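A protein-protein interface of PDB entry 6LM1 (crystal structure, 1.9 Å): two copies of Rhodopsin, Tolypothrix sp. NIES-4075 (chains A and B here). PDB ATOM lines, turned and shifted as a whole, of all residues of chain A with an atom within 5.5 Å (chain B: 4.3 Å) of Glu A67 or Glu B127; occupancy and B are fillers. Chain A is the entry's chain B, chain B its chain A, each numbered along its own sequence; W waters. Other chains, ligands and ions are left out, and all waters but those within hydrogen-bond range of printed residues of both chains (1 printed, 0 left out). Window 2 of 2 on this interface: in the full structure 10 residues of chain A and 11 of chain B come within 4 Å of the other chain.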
ATOM      1  N   LEU A  61     -30.136  -5.618 -27.658  1.00  0.00           N
ATOM      2  CA  LEU A  61     -29.797  -4.210 -27.464  1.00  0.00           C
ATOM      3  C   LEU A  61     -28.634  -3.780 -28.364  1.00  0.00           C
ATOM      4  O   LEU A  61     -28.661  -2.680 -28.924  1.00  0.00           O
ATOM      5  CB  LEU A  61     -29.486  -3.945 -25.987  1.00  0.00           C
ATOM      6  CG  LEU A  61     -29.257  -2.487 -25.579  1.00  0.00           C
ATOM      7  CD1 LEU A  61     -30.444  -1.594 -25.984  1.00  0.00           C
ATOM      8  CD2 LEU A  61     -29.003  -2.398 -24.076  1.00  0.00           C
ATOM      9  N   THR A  62     -27.602  -4.624 -28.526  1.00  0.00           N
ATOM     10  CA  THR A  62     -26.508  -4.216 -29.418  1.00  0.00           C
ATOM     11  C   THR A  62     -26.989  -4.058 -30.860  1.00  0.00           C
ATOM     12  O   THR A  62     -26.443  -3.238 -31.604  1.00  0.00           O
ATOM     13  CB  THR A  62     -25.326  -5.204 -29.380  1.00  0.00           C
ATOM     14  OG1 THR A  62     -25.739  -6.467 -29.905  1.00  0.00           O
ATOM     15  CG2 THR A  62     -24.800  -5.385 -27.965  1.00  0.00           C
ATOM     16  N   MET A  63     -28.008  -4.814 -31.271  1.00  0.00           N
ATOM     17  CA  MET A  63     -28.529  -4.652 -32.627  1.00  0.00           C
ATOM     18  C   MET A  63     -29.414  -3.409 -32.750  1.00  0.00           C
ATOM     19  O   MET A  63     -29.340  -2.690 -33.755  1.00  0.00           O
ATOM     20  CB  MET A  63     -29.278  -5.918 -33.047  1.00  0.00           C
ATOM     21  CG  MET A  63     -28.316  -7.098 -33.272  1.00  0.00           C
ATOM     22  SD  MET A  63     -29.044  -8.542 -34.074  1.00  0.00           S
ATOM     23  CE  MET A  63     -30.036  -9.230 -32.745  1.00  0.00           C
ATOM     24  N   LEU A  65     -28.956  -0.716 -31.206  1.00  0.00           N
ATOM     25  CA  LEU A  65     -28.008   0.391 -31.221  1.00  0.00           C
ATOM     26  C   LEU A  65     -27.094   0.381 -32.440  1.00  0.00           C
ATOM     27  O   LEU A  65     -26.245   1.270 -32.563  1.00  0.00           O
ATOM     28  CB  LEU A  65     -27.167   0.371 -29.939  1.00  0.00           C
ATOM     29  CG  LEU A  65     -27.958   0.601 -28.651  1.00  0.00           C
ATOM     30  CD1 LEU A  65     -27.078   0.318 -27.431  1.00  0.00           C
ATOM     31  CD2 LEU A  65     -28.503   2.020 -28.610  1.00  0.00           C
ATOM     32  N   GLY A  66     -27.254  -0.578 -33.348  1.00  0.00           N
ATOM     33  CA  GLY A  66     -26.422  -0.646 -34.534  1.00  0.00           C
ATOM     34  C   GLY A  66     -25.014  -1.147 -34.304  1.00  0.00           C
ATOM     35  O   GLY A  66     -24.180  -1.043 -35.212  1.00  0.00           O
ATOM     36  N   GLU A  67     -24.724  -1.700 -33.126  1.00  0.00           N
ATOM     37  CA  GLU A  67     -23.358  -2.107 -32.802  1.00  0.00           C
ATOM     38  C   GLU A  67     -22.976  -3.434 -33.454  1.00  0.00           C
ATOM     39  O   GLU A  67     -21.830  -3.604 -33.893  1.00  0.00           O
ATOM     40  CB  GLU A  67     -23.190  -2.186 -31.282  1.00  0.00           C
ATOM     41  CG  GLU A  67     -23.340  -0.821 -30.575  1.00  0.00           C
ATOM     42  CD  GLU A  67     -23.769  -0.950 -29.113  1.00  0.00           C
ATOM     43  OE1 GLU A  67     -24.128  -2.063 -28.682  1.00  0.00           O
ATOM     44  OE2 GLU A  67     -23.772   0.068 -28.395  1.00  0.00           O
ATOM     45  N   THR A  68     -23.896  -4.394 -33.508  1.00  0.00           N
ATOM     46  CA  THR A  68     -23.623  -5.705 -34.100  1.00  0.00           C
ATOM     47  C   THR A  68     -24.448  -5.911 -35.369  1.00  0.00           C
ATOM     48  O   THR A  68     -24.910  -7.013 -35.689  1.00  0.00           O
ATOM     49  CB  THR A  68     -23.867  -6.815 -33.085  1.00  0.00           C
ATOM     50  OG1 THR A  68     -25.219  -6.744 -32.631  1.00  0.00           O
ATOM     51  CG2 THR A  68     -22.924  -6.640 -31.877  1.00  0.00           C
ATOM     52  N   VAL A  69     -24.629  -4.821 -36.100  1.00  0.00           N
ATOM     53  CA  VAL A  69     -25.313  -4.802 -37.385  1.00  0.00           C
ATOM     54  C   VAL A  69     -24.407  -4.069 -38.363  1.00  0.00           C
ATOM     55  O   VAL A  69     -23.874  -3.003 -38.040  1.00  0.00           O
ATOM     56  CB  VAL A  69     -26.683  -4.107 -37.277  1.00  0.00           C
ATOM     57  CG1 VAL A  69     -27.292  -3.950 -38.635  1.00  0.00           C
ATOM     58  CG2 VAL A  69     -27.613  -4.893 -36.363  1.00  0.00           C
ATOM     59  N   TRP A  79     -25.330  -9.638 -37.589  1.00  0.00           N
ATOM     60  CA  TRP A  79     -24.411 -10.680 -37.135  1.00  0.00           C
ATOM     61  C   TRP A  79     -24.429 -10.848 -35.622  1.00  0.00           C
ATOM     62  O   TRP A  79     -23.968 -11.879 -35.115  1.00  0.00           O
ATOM     63  CB  TRP A  79     -22.987 -10.411 -37.629  1.00  0.00           C
ATOM     64  CG  TRP A  79     -22.411  -9.065 -37.305  1.00  0.00           C
ATOM     65  CD1 TRP A  79     -22.495  -7.932 -38.066  1.00  0.00           C
ATOM     66  CD2 TRP A  79     -21.624  -8.720 -36.157  1.00  0.00           C
ATOM     67  NE1 TRP A  79     -21.819  -6.903 -37.455  1.00  0.00           N
ATOM     68  CE2 TRP A  79     -21.276  -7.360 -36.283  1.00  0.00           C
ATOM     69  CE3 TRP A  79     -21.182  -9.431 -35.034  1.00  0.00           C
ATOM     70  CZ2 TRP A  79     -20.508  -6.693 -35.325  1.00  0.00           C
ATOM     71  CZ3 TRP A  79     -20.421  -8.764 -34.080  1.00  0.00           C
ATOM     72  CH2 TRP A  79     -20.096  -7.410 -34.233  1.00  0.00           C
ATOM     73  N   VAL B 123     -17.869  -2.838 -24.697  1.00  0.00           N
ATOM     74  CA  VAL B 123     -18.796  -2.098 -25.556  1.00  0.00           C
ATOM     75  C   VAL B 123     -18.904  -0.650 -25.094  1.00  0.00           C
ATOM     76  O   VAL B 123     -18.940   0.274 -25.916  1.00  0.00           O
ATOM     77  CB  VAL B 123     -20.181  -2.774 -25.600  1.00  0.00           C
ATOM     78  CG1 VAL B 123     -21.109  -1.960 -26.478  1.00  0.00           C
ATOM     79  CG2 VAL B 123     -20.061  -4.206 -26.137  1.00  0.00           C
ATOM     80  N   ALA B 124     -18.948  -0.424 -23.775  1.00  0.00           N
ATOM     81  CA  ALA B 124     -18.995   0.948 -23.270  1.00  0.00           C
ATOM     82  C   ALA B 124     -17.787   1.750 -23.741  1.00  0.00           C
ATOM     83  O   ALA B 124     -17.917   2.911 -24.142  1.00  0.00           O
ATOM     84  CB  ALA B 124     -19.055   0.950 -21.740  1.00  0.00           C
ATOM     85  N   THR B 125     -16.602   1.141 -23.688  1.00  0.00           N
ATOM     86  CA  THR B 125     -15.374   1.814 -24.090  1.00  0.00           C
ATOM     87  C   THR B 125     -15.370   2.115 -25.585  1.00  0.00           C
ATOM     88  O   THR B 125     -14.900   3.174 -26.012  1.00  0.00           O
ATOM     89  CB  THR B 125     -14.183   0.932 -23.703  1.00  0.00           C
ATOM     90  OG1 THR B 125     -14.205   0.712 -22.288  1.00  0.00           O
ATOM     91  CG2 THR B 125     -12.853   1.558 -24.105  1.00  0.00           C
ATOM     92  N   LEU B 126     -15.892   1.201 -26.398  1.00  0.00           N
ATOM     93  CA  LEU B 126     -15.906   1.431 -27.840  1.00  0.00           C
ATOM     94  C   LEU B 126     -16.994   2.401 -28.279  1.00  0.00           C
ATOM     95  O   LEU B 126     -16.895   2.967 -29.374  1.00  0.00           O
ATOM     96  CB  LEU B 126     -16.071   0.105 -28.575  1.00  0.00           C
ATOM     97  CG  LEU B 126     -14.969  -0.920 -28.316  1.00  0.00           C
ATOM     98  CD1 LEU B 126     -15.326  -2.228 -28.980  1.00  0.00           C
ATOM     99  CD2 LEU B 126     -13.614  -0.412 -28.824  1.00  0.00           C
ATOM    100  N   GLU B 127     -18.010   2.632 -27.457  1.00  0.00           N
ATOM    101  CA  GLU B 127     -19.144   3.436 -27.892  1.00  0.00           C
ATOM    102  C   GLU B 127     -18.887   4.924 -27.668  1.00  0.00           C
ATOM    103  O   GLU B 127     -17.921   5.333 -27.026  1.00  0.00           O
ATOM    104  CB  GLU B 127     -20.419   3.016 -27.157  1.00  0.00           C
ATOM    105  CG  GLU B 127     -21.328   2.093 -27.948  1.00  0.00           C
ATOM    106  CD  GLU B 127     -22.079   2.796 -29.077  1.00  0.00           C
ATOM    107  OE1 GLU B 127     -21.815   3.981 -29.355  1.00  0.00           O
ATOM    108  OE2 GLU B 127     -22.946   2.157 -29.696  1.00  0.00           O
ATOM    109  N   ALA B 128     -19.781   5.736 -28.213  1.00  0.00           N
ATOM    110  CA  ALA B 128     -19.778   7.173 -28.009  1.00  0.00           C
ATOM    111  C   ALA B 128     -20.852   7.567 -26.998  1.00  0.00           C
ATOM    112  O   ALA B 128     -21.847   6.855 -26.832  1.00  0.00           O
ATOM    113  CB  ALA B 128     -20.023   7.898 -29.337  1.00  0.00           C
ATOM    114  N   THR B 131     -24.517   6.672 -25.368  1.00  0.00           N
ATOM    115  CA  THR B 131     -24.686   5.222 -25.431  1.00  0.00           C
ATOM    116  C   THR B 131     -23.647   4.514 -24.579  1.00  0.00           C
ATOM    117  O   THR B 131     -23.945   3.500 -23.935  1.00  0.00           O
ATOM    118  CB  THR B 131     -24.607   4.754 -26.882  1.00  0.00           C
ATOM    119  OG1 THR B 131     -25.424   5.607 -27.686  1.00  0.00           O
ATOM    120  CG2 THR B 131     -25.104   3.311 -27.013  1.00  0.00           C
ATOM    121  N   SER B 132     -22.427   5.052 -24.537  1.00  0.00           N
ATOM    122  CA  SER B 132     -21.379   4.443 -23.728  1.00  0.00           C
ATOM    123  C   SER B 132     -21.794   4.358 -22.270  1.00  0.00           C
ATOM    124  O   SER B 132     -21.472   3.387 -21.578  1.00  0.00           O
ATOM    125  CB  SER B 132     -20.092   5.250 -23.865  1.00  0.00           C
ATOM    126  OG  SER B 132     -20.349   6.624 -23.619  1.00  0.00           O
ATOM    127  N   TRP B 135     -24.052   1.302 -21.416  1.00  0.00           N
ATOM    128  CA  TRP B 135     -23.336   0.047 -21.204  1.00  0.00           C
ATOM    129  C   TRP B 135     -22.526   0.071 -19.915  1.00  0.00           C
ATOM    130  O   TRP B 135     -22.358  -0.971 -19.271  1.00  0.00           O
ATOM    131  CB  TRP B 135     -22.438  -0.238 -22.401  1.00  0.00           C
ATOM    132  CG  TRP B 135     -23.247  -0.639 -23.594  1.00  0.00           C
ATOM    133  CD1 TRP B 135     -23.473   0.091 -24.720  1.00  0.00           C
ATOM    134  CD2 TRP B 135     -23.977  -1.859 -23.748  1.00  0.00           C
ATOM    135  NE1 TRP B 135     -24.284  -0.614 -25.588  1.00  0.00           N
ATOM    136  CE2 TRP B 135     -24.614  -1.811 -25.004  1.00  0.00           C
ATOM    137  CE3 TRP B 135     -24.154  -2.992 -22.938  1.00  0.00           C
ATOM    138  CZ2 TRP B 135     -25.410  -2.859 -25.482  1.00  0.00           C
ATOM    139  CZ3 TRP B 135     -24.945  -4.033 -23.414  1.00  0.00           C
ATOM    140  CH2 TRP B 135     -25.562  -3.954 -24.677  1.00  0.00           C
HETATM  141  O   HOH W   1     -24.238   3.039 -31.741  1.00  0.00           O
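OE2 of Glu A67 lies close to OE2 of Glu B127 (2.6 Å). OE2 of Glu A67 sits at hydrogen-bond distance from NE1 of Trp B135 (2.9 Å).
O of Thr A62 is in hydrogen-bond range of N of Glu A67 (2.8 Å). OG1 of Thr A62 lies within hydrogen-bond range of OG1 of Thr A68, at 2.8 Å.
Leu A61 touches Trp B135. Trp B135 touches Thr A62. CG2 of Thr B131 touches CD1 of Leu A65, 3.6 Å away. Leu A65 touches Trp B135. Val B123 touches Glu A67 (CG1 to OE1, 3.7 Å). Glu A67 touches Thr B131 (OE2 to CG2, 3.8 Å).
Glu A67 touches just these residues of chain B: Val B123 (3.7 Å), Glu B127 (2.6 Å), Thr B131 (3.8 Å) and Trp B135 (2.9 Å). Glu B127 touches just one residue of chain A: Glu A67. Printed residues of chain A within 4 Å of Thr B131: Leu A65 and Glu A67. Of the printed residues of chain A, Val B123 touches Glu A67 (3.7 Å). Of the printed residues of chain B, Leu A65 touches Thr B131 and Trp B135. The nearest printed residue of chain A that does not touch Thr B131 is Leu A61 (7.2 Å).
Hydrophobic or aromatic side chains of chain B that line the printed part of chain A: Val B123 and Trp B135. Hydrophobic or aromatic side chains of chain A that line the printed part of chain B: Leu A61 and Leu A65. Along chain A the printed residues that touch a printed residue of chain B span positions 61 to 67. Among the printed residues, 8 pairs touch across the chains. Among the printed residues, no Asp or Glu carboxylate lies within 4 Å of a Lys or Arg side-chain nitrogen of the other chain.
No position is printed for both chains. Of the 8 pairs that touch across the chains among the printed residues, none has its exchanged pair printed and touching as well.
Water W1 bridges OE2 of Glu B127 and O of Leu A65.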
